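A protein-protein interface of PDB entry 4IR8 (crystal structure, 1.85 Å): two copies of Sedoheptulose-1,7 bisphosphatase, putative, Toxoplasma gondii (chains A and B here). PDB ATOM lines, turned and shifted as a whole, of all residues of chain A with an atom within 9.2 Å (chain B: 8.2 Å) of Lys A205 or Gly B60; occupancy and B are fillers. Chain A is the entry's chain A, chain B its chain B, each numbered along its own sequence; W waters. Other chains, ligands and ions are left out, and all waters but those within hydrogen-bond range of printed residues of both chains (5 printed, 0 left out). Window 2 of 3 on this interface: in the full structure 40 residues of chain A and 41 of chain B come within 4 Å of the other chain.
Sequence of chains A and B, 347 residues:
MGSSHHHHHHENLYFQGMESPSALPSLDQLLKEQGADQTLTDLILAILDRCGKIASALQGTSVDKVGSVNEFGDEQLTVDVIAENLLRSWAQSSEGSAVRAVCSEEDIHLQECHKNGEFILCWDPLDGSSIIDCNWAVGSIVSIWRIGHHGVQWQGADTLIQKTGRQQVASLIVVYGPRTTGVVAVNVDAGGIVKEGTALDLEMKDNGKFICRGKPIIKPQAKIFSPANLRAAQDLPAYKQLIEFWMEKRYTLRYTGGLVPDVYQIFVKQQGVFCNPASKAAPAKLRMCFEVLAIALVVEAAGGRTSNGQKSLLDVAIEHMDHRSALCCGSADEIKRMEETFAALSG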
ATOM      1  N   LEU A  24      25.333  -8.368  23.960  1.00  0.00           N
ATOM      2  CA  LEU A  24      24.945  -8.676  22.551  1.00  0.00           C
ATOM      3  C   LEU A  24      25.079  -7.428  21.671  1.00  0.00           C
ATOM      4  O   LEU A  24      24.693  -6.337  22.086  1.00  0.00           O
ATOM      5  CB  LEU A  24      23.515  -9.214  22.499  1.00  0.00           C
ATOM      6  CG  LEU A  24      23.295 -10.549  23.213  1.00  0.00           C
ATOM      7  CD1 LEU A  24      21.811 -10.877  23.277  1.00  0.00           C
ATOM      8  CD2 LEU A  24      24.082 -11.669  22.530  1.00  0.00           C
ATOM      9  N   GLY A  52       7.435   0.677  14.958  1.00  0.00           N
ATOM     10  CA  GLY A  52       7.071   0.543  16.379  1.00  0.00           C
ATOM     11  C   GLY A  52       5.769   1.282  16.690  1.00  0.00           C
ATOM     12  O   GLY A  52       4.906   0.796  17.452  1.00  0.00           O
ATOM     13  N   ALA A  55       2.876  -0.614  15.299  1.00  0.00           N
ATOM     14  CA  ALA A  55       2.560  -1.688  16.247  1.00  0.00           C
ATOM     15  C   ALA A  55       1.631  -1.169  17.349  1.00  0.00           C
ATOM     16  O   ALA A  55       0.620  -1.795  17.680  1.00  0.00           O
ATOM     17  CB  ALA A  55       3.852  -2.276  16.874  1.00  0.00           C
ATOM     18  N   SER A  56       1.953   0.002  17.895  1.00  0.00           N
ATOM     19  CA  SER A  56       1.104   0.623  18.913  1.00  0.00           C
ATOM     20  C   SER A  56      -0.286   0.989  18.372  1.00  0.00           C
ATOM     21  O   SER A  56      -1.302   0.852  19.083  1.00  0.00           O
ATOM     22  CB  SER A  56       1.774   1.861  19.503  1.00  0.00           C
ATOM     23  OG  SER A  56       2.942   1.516  20.206  1.00  0.00           O
ATOM     24  N   GLN A  59      -2.367  -2.038  18.406  1.00  0.00           N
ATOM     25  CA  GLN A  59      -2.669  -2.466  19.783  1.00  0.00           C
ATOM     26  C   GLN A  59      -3.754  -1.642  20.471  1.00  0.00           C
ATOM     27  O   GLN A  59      -4.528  -2.173  21.269  1.00  0.00           O
ATOM     28  CB  GLN A  59      -1.399  -2.378  20.648  1.00  0.00           C
ATOM     29  CG  GLN A  59      -0.261  -3.295  20.226  1.00  0.00           C
ATOM     30  CD  GLN A  59       1.081  -2.939  20.875  1.00  0.00           C
ATOM     31  OE1 GLN A  59       1.161  -2.065  21.735  1.00  0.00           O
ATOM     32  NE2 GLN A  59       2.144  -3.611  20.440  1.00  0.00           N
ATOM     33  N   GLY A 177       2.615  -9.213  15.291  1.00  0.00           N
ATOM     34  CA  GLY A 177       1.921 -10.360  15.865  1.00  0.00           C
ATOM     35  C   GLY A 177       1.878 -10.131  17.363  1.00  0.00           C
ATOM     36  O   GLY A 177       1.807  -8.987  17.816  1.00  0.00           O
ATOM     37  N   PRO A 178       1.937 -11.199  18.148  1.00  0.00           N
ATOM     38  CA  PRO A 178       2.008 -11.000  19.601  1.00  0.00           C
ATOM     39  C   PRO A 178       3.239 -10.168  19.986  1.00  0.00           C
ATOM     40  O   PRO A 178       3.209  -9.436  20.963  1.00  0.00           O
ATOM     41  CB  PRO A 178       2.111 -12.421  20.159  1.00  0.00           C
ATOM     42  CG  PRO A 178       1.806 -13.320  19.076  1.00  0.00           C
ATOM     43  CD  PRO A 178       1.958 -12.615  17.767  1.00  0.00           C
ATOM     44  N   ARG A 179       4.320 -10.332  19.223  1.00  0.00           N
ATOM     45  CA  ARG A 179       5.553  -9.552  19.357  1.00  0.00           C
ATOM     46  C   ARG A 179       5.622  -8.737  18.077  1.00  0.00           C
ATOM     47  O   ARG A 179       4.723  -8.834  17.238  1.00  0.00           O
ATOM     48  CB  ARG A 179       6.800 -10.470  19.378  1.00  0.00           C
ATOM     49  CG  ARG A 179       7.014 -11.241  20.638  1.00  0.00           C
ATOM     50  CD  ARG A 179       8.242 -12.173  20.583  1.00  0.00           C
ATOM     51  NE  ARG A 179       7.990 -13.344  19.757  1.00  0.00           N
ATOM     52  CZ  ARG A 179       8.682 -13.725  18.685  1.00  0.00           C
ATOM     53  NH1 ARG A 179       9.798 -13.101  18.318  1.00  0.00           N
ATOM     54  NH2 ARG A 179       8.292 -14.813  18.021  1.00  0.00           N
ATOM     55  N   THR A 180       6.671  -7.929  17.931  1.00  0.00           N
ATOM     56  CA  THR A 180       6.913  -7.207  16.686  1.00  0.00           C
ATOM     57  C   THR A 180       8.285  -7.663  16.254  1.00  0.00           C
ATOM     58  O   THR A 180       9.256  -7.545  17.015  1.00  0.00           O
ATOM     59  CB  THR A 180       6.850  -5.700  16.852  1.00  0.00           C
ATOM     60  OG1 THR A 180       5.569  -5.334  17.366  1.00  0.00           O
ATOM     61  CG2 THR A 180       7.060  -5.021  15.512  1.00  0.00           C
ATOM     62  N   THR A 181       8.370  -8.233  15.055  1.00  0.00           N
ATOM     63  CA  THR A 181       9.627  -8.778  14.569  1.00  0.00           C
ATOM     64  C   THR A 181       9.861  -8.283  13.167  1.00  0.00           C
ATOM     65  O   THR A 181       9.077  -7.511  12.638  1.00  0.00           O
ATOM     66  CB  THR A 181       9.592 -10.321  14.585  1.00  0.00           C
ATOM     67  OG1 THR A 181       8.507 -10.762  13.757  1.00  0.00           O
ATOM     68  CG2 THR A 181       9.402 -10.853  16.001  1.00  0.00           C
ATOM     69  N   LEU A 202      14.999  -9.749  13.334  1.00  0.00           N
ATOM     70  CA  LEU A 202      14.803  -8.743  14.345  1.00  0.00           C
ATOM     71  C   LEU A 202      13.629  -8.974  15.281  1.00  0.00           C
ATOM     72  O   LEU A 202      12.626  -9.579  14.903  1.00  0.00           O
ATOM     73  CB  LEU A 202      14.565  -7.419  13.656  1.00  0.00           C
ATOM     74  CG  LEU A 202      15.572  -6.916  12.617  1.00  0.00           C
ATOM     75  CD1 LEU A 202      15.021  -5.633  12.045  1.00  0.00           C
ATOM     76  CD2 LEU A 202      16.982  -6.702  13.189  1.00  0.00           C
ATOM     77  N   GLU A 203      13.754  -8.416  16.484  1.00  0.00           N
ATOM     78  CA  GLU A 203      12.719  -8.471  17.503  1.00  0.00           C
ATOM     79  C   GLU A 203      12.659  -7.137  18.267  1.00  0.00           C
ATOM     80  O   GLU A 203      13.679  -6.620  18.717  1.00  0.00           O
ATOM     81  CB  GLU A 203      12.998  -9.609  18.466  1.00  0.00           C
ATOM     82  CG  GLU A 203      11.987  -9.750  19.570  1.00  0.00           C
ATOM     83  CD  GLU A 203      12.261 -10.954  20.402  1.00  0.00           C
ATOM     84  OE1 GLU A 203      12.808 -10.783  21.505  1.00  0.00           O
ATOM     85  OE2 GLU A 203      12.012 -12.076  19.918  1.00  0.00           O
ATOM     86  N   MET A 204      11.463  -6.591  18.439  1.00  0.00           N
ATOM     87  CA  MET A 204      11.336  -5.343  19.152  1.00  0.00           C
ATOM     88  C   MET A 204      11.280  -5.538  20.669  1.00  0.00           C
ATOM     89  O   MET A 204      10.587  -6.439  21.183  1.00  0.00           O
ATOM     90  CB  MET A 204      10.082  -4.589  18.695  1.00  0.00           C
ATOM     91  CG  MET A 204      10.002  -3.164  19.108  1.00  0.00           C
ATOM     92  SD  MET A 204       8.480  -2.347  18.497  1.00  0.00           S
ATOM     93  CE  MET A 204       7.275  -2.885  19.687  1.00  0.00           C
ATOM     94  N   LYS A 205      11.987  -4.667  21.381  1.00  0.00           N
ATOM     95  CA  LYS A 205      11.922  -4.607  22.841  1.00  0.00           C
ATOM     96  C   LYS A 205      11.203  -3.292  23.131  1.00  0.00           C
ATOM     97  O   LYS A 205      10.076  -3.111  22.689  1.00  0.00           O
ATOM     98  CB  LYS A 205      13.308  -4.679  23.471  1.00  0.00           C
ATOM     99  CG  LYS A 205      13.958  -6.052  23.325  1.00  0.00           C
ATOM    100  CD  LYS A 205      13.065  -7.140  23.902  1.00  0.00           C
ATOM    101  CE  LYS A 205      13.650  -8.530  23.694  1.00  0.00           C
ATOM    102  NZ  LYS A 205      12.700  -9.597  24.130  1.00  0.00           N
ATOM    103  N   ASP A 206      11.830  -2.357  23.840  1.00  0.00           N
ATOM    104  CA  ASP A 206      11.173  -1.064  24.074  1.00  0.00           C
ATOM    105  C   ASP A 206      10.650  -0.524  22.737  1.00  0.00           C
ATOM    106  O   ASP A 206      11.392  -0.427  21.754  1.00  0.00           O
ATOM    107  CB  ASP A 206      12.137  -0.069  24.697  1.00  0.00           C
ATOM    108  CG  ASP A 206      12.678  -0.540  26.015  1.00  0.00           C
ATOM    109  OD1 ASP A 206      13.630   0.084  26.506  1.00  0.00           O
ATOM    110  OD2 ASP A 206      12.154  -1.535  26.560  1.00  0.00           O
ATOM    111  N   ASN A 207       9.377  -0.150  22.706  1.00  0.00           N
ATOM    112  CA  ASN A 207       8.756   0.285  21.460  1.00  0.00           C
ATOM    113  C   ASN A 207       9.711   1.011  20.512  1.00  0.00           C
ATOM    114  O   ASN A 207      10.432   1.925  20.907  1.00  0.00           O
ATOM    115  CB  ASN A 207       7.555   1.186  21.719  1.00  0.00           C
ATOM    116  CG  ASN A 207       6.737   1.414  20.468  1.00  0.00           C
ATOM    117  OD1 ASN A 207       6.883   2.438  19.804  1.00  0.00           O
ATOM    118  ND2 ASN A 207       5.905   0.426  20.103  1.00  0.00           N
ATOM    119  N   GLY A 208       9.700   0.578  19.257  1.00  0.00           N
ATOM    120  CA  GLY A 208      10.505   1.168  18.206  1.00  0.00           C
ATOM    121  C   GLY A 208      11.974   0.755  18.182  1.00  0.00           C
ATOM    122  O   GLY A 208      12.663   1.066  17.208  1.00  0.00           O
ATOM    123  N   LYS A 209      12.452   0.062  19.226  1.00  0.00           N
ATOM    124  CA  LYS A 209      13.862  -0.376  19.306  1.00  0.00           C
ATOM    125  C   LYS A 209      14.024  -1.900  19.187  1.00  0.00           C
ATOM    126  O   LYS A 209      13.473  -2.674  19.978  1.00  0.00           O
ATOM    127  CB  LYS A 209      14.529   0.121  20.572  1.00  0.00           C
ATOM    128  CG  LYS A 209      14.727   1.639  20.564  1.00  0.00           C
ATOM    129  CD  LYS A 209      15.860   2.086  21.458  1.00  0.00           C
ATOM    130  CE  LYS A 209      16.188   3.563  21.210  1.00  0.00           C
ATOM    131  NZ  LYS A 209      17.528   3.955  21.739  1.00  0.00           N
ATOM    132  N   PHE A 210      14.814  -2.305  18.200  1.00  0.00           N
ATOM    133  CA  PHE A 210      14.956  -3.700  17.850  1.00  0.00           C
ATOM    134  C   PHE A 210      16.325  -4.281  18.157  1.00  0.00           C
ATOM    135  O   PHE A 210      17.336  -3.584  18.136  1.00  0.00           O
ATOM    136  CB  PHE A 210      14.678  -3.869  16.354  1.00  0.00           C
ATOM    137  CG  PHE A 210      13.233  -3.625  15.962  1.00  0.00           C
ATOM    138  CD1 PHE A 210      12.725  -2.331  15.894  1.00  0.00           C
ATOM    139  CD2 PHE A 210      12.398  -4.685  15.651  1.00  0.00           C
ATOM    140  CE1 PHE A 210      11.395  -2.108  15.503  1.00  0.00           C
ATOM    141  CE2 PHE A 210      11.080  -4.470  15.270  1.00  0.00           C
ATOM    142  CZ  PHE A 210      10.584  -3.164  15.206  1.00  0.00           C
ATOM    143  N   ILE A 211      16.330  -5.571  18.468  1.00  0.00           N
ATOM    144  CA  ILE A 211      17.554  -6.309  18.650  1.00  0.00           C
ATOM    145  C   ILE A 211      17.580  -7.373  17.568  1.00  0.00           C
ATOM    146  O   ILE A 211      16.550  -7.645  16.921  1.00  0.00           O
ATOM    147  CB  ILE A 211      17.705  -6.951  20.059  1.00  0.00           C
ATOM    148  CG1 ILE A 211      16.603  -7.978  20.348  1.00  0.00           C
ATOM    149  CG2 ILE A 211      17.800  -5.848  21.136  1.00  0.00           C
ATOM    150  CD1 ILE A 211      16.843  -8.799  21.619  1.00  0.00           C
ATOM    151  N   CYS A 212      18.754  -7.933  17.320  1.00  0.00           N
ATOM    152  CA  CYS A 212      18.887  -9.004  16.331  1.00  0.00           C
ATOM    153  C   CYS A 212      18.780 -10.348  17.039  1.00  0.00           C
ATOM    154  O   CYS A 212      19.497 -10.581  18.015  1.00  0.00           O
ATOM    155  CB  CYS A 212      20.228  -8.896  15.609  1.00  0.00           C
ATOM    156  SG  CYS A 212      20.490 -10.147  14.341  1.00  0.00           S
ATOM    157  N   ARG A 213      17.882 -11.208  16.546  1.00  0.00           N
ATOM    158  CA  ARG A 213      17.657 -12.540  17.127  1.00  0.00           C
ATOM    159  C   ARG A 213      18.355 -13.667  16.347  1.00  0.00           C
ATOM    160  O   ARG A 213      18.219 -14.835  16.714  1.00  0.00           O
ATOM    161  CB  ARG A 213      16.152 -12.830  17.326  1.00  0.00           C
ATOM    162  CG  ARG A 213      15.301 -12.825  16.043  1.00  0.00           C
ATOM    163  CD  ARG A 213      13.820 -13.186  16.316  1.00  0.00           C
ATOM    164  NE  ARG A 213      13.706 -14.427  17.086  1.00  0.00           N
ATOM    165  CZ  ARG A 213      13.638 -15.656  16.577  1.00  0.00           C
ATOM    166  NH1 ARG A 213      13.645 -15.870  15.262  1.00  0.00           N
ATOM    167  NH2 ARG A 213      13.563 -16.695  17.404  1.00  0.00           N
ATOM    168  N   LYS B  53      -2.592 -11.031  30.864  1.00  0.00           N
ATOM    169  CA  LYS B  53      -1.231 -11.136  31.365  1.00  0.00           C
ATOM    170  C   LYS B  53      -0.380 -12.061  30.462  1.00  0.00           C
ATOM    171  O   LYS B  53       0.815 -11.812  30.271  1.00  0.00           O
ATOM    172  CB  LYS B  53      -1.249 -11.535  32.840  1.00  0.00           C
ATOM    173  CG  LYS B  53      -1.747 -10.356  33.714  1.00  0.00           C
ATOM    174  CD  LYS B  53      -2.060 -10.728  35.131  1.00  0.00           C
ATOM    175  CE  LYS B  53      -2.233  -9.471  36.008  1.00  0.00           C
ATOM    176  NZ  LYS B  53      -3.199  -8.471  35.425  1.00  0.00           N
ATOM    177  N   ILE B  54      -0.998 -13.088  29.875  1.00  0.00           N
ATOM    178  CA  ILE B  54      -0.296 -13.942  28.917  1.00  0.00           C
ATOM    179  C   ILE B  54       0.051 -13.077  27.699  1.00  0.00           C
ATOM    180  O   ILE B  54       1.184 -13.124  27.181  1.00  0.00           O
ATOM    181  CB  ILE B  54      -1.138 -15.183  28.521  1.00  0.00           C
ATOM    182  CG1 ILE B  54      -1.313 -16.098  29.739  1.00  0.00           C
ATOM    183  CG2 ILE B  54      -0.479 -15.934  27.385  1.00  0.00           C
ATOM    184  CD1 ILE B  54      -2.297 -17.234  29.543  1.00  0.00           C
ATOM    185  N   ALA B  55      -0.890 -12.232  27.280  1.00  0.00           N
ATOM    186  CA  ALA B  55      -0.640 -11.334  26.141  1.00  0.00           C
ATOM    187  C   ALA B  55       0.601 -10.458  26.383  1.00  0.00           C
ATOM    188  O   ALA B  55       1.422 -10.260  25.476  1.00  0.00           O
ATOM    189  CB  ALA B  55      -1.861 -10.470  25.854  1.00  0.00           C
ATOM    190  N   SER B  56       0.736  -9.933  27.600  1.00  0.00           N
ATOM    191  CA  SER B  56       1.920  -9.139  27.970  1.00  0.00           C
ATOM    192  C   SER B  56       3.197  -9.949  27.961  1.00  0.00           C
ATOM    193  O   SER B  56       4.215  -9.478  27.464  1.00  0.00           O
ATOM    194  CB  SER B  56       1.746  -8.483  29.344  1.00  0.00           C
ATOM    195  OG  SER B  56       0.769  -7.469  29.273  1.00  0.00           O
ATOM    196  N   ALA B  57       3.158 -11.156  28.518  1.00  0.00           N
ATOM    197  CA  ALA B  57       4.324 -12.029  28.542  1.00  0.00           C
ATOM    198  C   ALA B  57       4.809 -12.290  27.124  1.00  0.00           C
ATOM    199  O   ALA B  57       5.999 -12.224  26.853  1.00  0.00           O
ATOM    200  CB  ALA B  57       3.993 -13.356  29.238  1.00  0.00           C
ATOM    201  N   LEU B  58       3.882 -12.579  26.210  1.00  0.00           N
ATOM    202  CA  LEU B  58       4.252 -12.852  24.809  1.00  0.00           C
ATOM    203  C   LEU B  58       4.942 -11.674  24.121  1.00  0.00           C
ATOM    204  O   LEU B  58       5.882 -11.850  23.335  1.00  0.00           O
ATOM    205  CB  LEU B  58       3.004 -13.229  23.995  1.00  0.00           C
ATOM    206  CG  LEU B  58       2.335 -14.545  24.372  1.00  0.00           C
ATOM    207  CD1 LEU B  58       0.974 -14.762  23.602  1.00  0.00           C
ATOM    208  CD2 LEU B  58       3.267 -15.709  24.124  1.00  0.00           C
ATOM    209  N   GLN B  59       4.460 -10.478  24.419  1.00  0.00           N
ATOM    210  CA  GLN B  59       4.960  -9.251  23.814  1.00  0.00           C
ATOM    211  C   GLN B  59       6.390  -8.898  24.232  1.00  0.00           C
ATOM    212  O   GLN B  59       7.139  -8.292  23.454  1.00  0.00           O
ATOM    213  CB  GLN B  59       3.980  -8.146  24.177  1.00  0.00           C
ATOM    214  CG  GLN B  59       4.165  -6.816  23.520  1.00  0.00           C
ATOM    215  CD  GLN B  59       2.950  -5.921  23.757  1.00  0.00           C
ATOM    216  OE1 GLN B  59       3.007  -4.708  23.565  1.00  0.00           O
ATOM    217  NE2 GLN B  59       1.843  -6.527  24.199  1.00  0.00           N
ATOM    218  N   GLY B  60       6.785  -9.311  25.435  1.00  0.00           N
ATOM    219  CA  GLY B  60       8.125  -9.004  25.942  1.00  0.00           C
ATOM    220  C   GLY B  60       9.104 -10.155  26.094  1.00  0.00           C
ATOM    221  O   GLY B  60      10.279  -9.928  26.422  1.00  0.00           O
ATOM    222  N   THR B  61       8.655 -11.385  25.848  1.00  0.00           N
ATOM    223  CA  THR B  61       9.520 -12.555  26.002  1.00  0.00           C
ATOM    224  C   THR B  61      10.002 -13.086  24.655  1.00  0.00           C
ATOM    225  O   THR B  61       9.194 -13.413  23.782  1.00  0.00           O
ATOM    226  CB  THR B  61       8.790 -13.692  26.756  1.00  0.00           C
ATOM    227  OG1 THR B  61       8.268 -13.190  27.996  1.00  0.00           O
ATOM    228  CG2 THR B  61       9.741 -14.864  27.030  1.00  0.00           C
ATOM    229  N   SER B  62      11.324 -13.176  24.497  1.00  0.00           N
ATOM    230  CA  SER B  62      11.917 -13.711  23.278  1.00  0.00           C
ATOM    231  C   SER B  62      11.629 -15.212  23.152  1.00  0.00           C
ATOM    232  O   SER B  62      11.132 -15.853  24.091  1.00  0.00           O
ATOM    233  CB  SER B  62      13.441 -13.506  23.286  1.00  0.00           C
ATOM    234  OG  SER B  62      13.807 -12.139  23.427  1.00  0.00           O
ATOM    235  N   VAL B  63      11.924 -15.764  21.979  1.00  0.00           N
ATOM    236  CA  VAL B  63      11.804 -17.199  21.752  1.00  0.00           C
ATOM    237  C   VAL B  63      13.033 -17.853  22.394  1.00  0.00           C
ATOM    238  O   VAL B  63      14.151 -17.729  21.887  1.00  0.00           O
ATOM    239  CB  VAL B  63      11.737 -17.532  20.248  1.00  0.00           C
ATOM    240  CG1 VAL B  63      12.007 -19.017  19.999  1.00  0.00           C
ATOM    241  CG2 VAL B  63      10.386 -17.102  19.673  1.00  0.00           C
ATOM    242  N   VAL B  79       7.818 -19.195  27.167  1.00  0.00           N
ATOM    243  CA  VAL B  79       6.485 -18.581  27.158  1.00  0.00           C
ATOM    244  C   VAL B  79       5.356 -19.570  27.471  1.00  0.00           C
ATOM    245  O   VAL B  79       4.369 -19.182  28.075  1.00  0.00           O
ATOM    246  CB  VAL B  79       6.187 -17.832  25.836  1.00  0.00           C
ATOM    247  CG1 VAL B  79       7.090 -16.598  25.717  1.00  0.00           C
ATOM    248  CG2 VAL B  79       6.360 -18.751  24.643  1.00  0.00           C
ATOM    249  N   ILE B  82       5.470 -19.960  31.207  1.00  0.00           N
ATOM    250  CA  ILE B  82       5.005 -18.706  31.799  1.00  0.00           C
ATOM    251  C   ILE B  82       3.470 -18.629  31.705  1.00  0.00           C
ATOM    252  O   ILE B  82       2.808 -18.280  32.676  1.00  0.00           O
ATOM    253  CB  ILE B  82       5.634 -17.481  31.112  1.00  0.00           C
ATOM    254  CG1 ILE B  82       7.138 -17.423  31.414  1.00  0.00           C
ATOM    255  CG2 ILE B  82       4.956 -16.194  31.587  1.00  0.00           C
ATOM    256  CD1 ILE B  82       7.861 -16.271  30.779  1.00  0.00           C
HETATM  257  O   HOH W   1       6.454 -14.392  22.341  1.00  0.00           O
HETATM  258  O   HOH W   2      13.331 -14.323  19.942  1.00  0.00           O
HETATM  259  O   HOH W   3       0.791 -10.183  22.823  1.00  0.00           O
HETATM  260  O   HOH W   4       8.033  -7.388  20.398  1.00  0.00           O
HETATM  261  O   HOH W   5      10.011  -8.772  22.746  1.00  0.00           O
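Water W2 lies within hydrogen-bond range of the side-chain carboxylate (OE2) of Glu A203 (2.6 Å), the backbone NH (N) of Val B63 (2.9 Å) and the guanidinium group (NE) of Arg A213 (2.9 Å).
Water W3 bridges O of Ala B55 (2.7 Å) and O of Pro A178 (3.1 Å).
Water W1 lies within hydrogen-bond range of O of Leu B58 (2.8 Å), NE of Arg A179 (3.2 Å) and O of Thr B61 (3.2 Å).
Water W4 lies within hydrogen-bond range of the backbone carbonyl oxygen (O) of Met A204, the backbone NH (N) of Thr A180 and the backbone carbonyl oxygen (O) of Gln B59.
Water W5 lies within hydrogen-bond range of the backbone carbonyl oxygen (O) of Met A204 (2.9 Å), the backbone carbonyl oxygen (O) of Gln B59 (3.0 Å) and the side-chain amino group (NZ) of Lys A205 (3.1 Å).
The side-chain amide oxygen of Gln B59 lies within hydrogen-bond range of the side-chain amide nitrogen of Gln A59, 3.4 Å away.
OG of Ser B62 sits at hydrogen-bond distance from OE1 of Glu A203 (2.6 Å).
NZ of Lys A205 is in hydrogen-bond range of O of Gly B60.
The side-chain amino group of Lys A205 is in hydrogen-bond range of the side-chain hydroxyl of Ser B62, at 2.9 Å.
O of Pro A178 touches CA of Gln B59, at 3.4 Å.
Arg A179 touches Leu B58.
Thr B61 touches Arg A179 (O to CD, 3.6 Å).
Val B63 touches Arg A179 (CG2 to NH2, 3.5 Å).
Val B63 touches Arg A213 (CB to NH2, 3.5 Å).
The side-chain carboxylate (OE2) of Glu A203 is in salt-bridge range of the guanidinium group (NH1) of Arg A179 (2.9 Å).
The side-chain carboxylate of Glu A203 lies within salt-bridge range of the side-chain amino group of Lys A205 (2.9 Å).
N of Ile A211 is in hydrogen-bond range of O of Glu A203 (2.9 Å).
The backbone carbonyl oxygen of Ala B57 is in hydrogen-bond range of the side-chain hydroxyl of Thr B61 (2.7 Å).
Printed residues of chain B within 4 Å of Pro A178: Gln B59 (3.4 Å).
Of the printed residues of chain B, Lys A205 touches Gly B60 (3.4 Å) and Ser B62 (2.9 Å).
Printed residues of chain A within 4 Å of Gly B60: Lys A205.
Of the printed residues of chain A, Val B63 touches Arg A179 and Arg A213.
Gln A59 touches its own counterpart, Gln B59.
Positions printed for both chains: 55, 56 and 59.
Of the 9 pairs that touch across the chains among the printed residues, 1 has its exchanged pair printed and touching as well.
Of the 13 printed residues of chain B, 6 touch a printed residue of chain A.
Hydrophobic or aromatic side chains of chain B within 4 Å of the printed part of chain A: Val B63.
Among the printed residues, no Asp or Glu carboxylate lies within 4 Å of a Lys or Arg side-chain nitrogen of the other chain.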
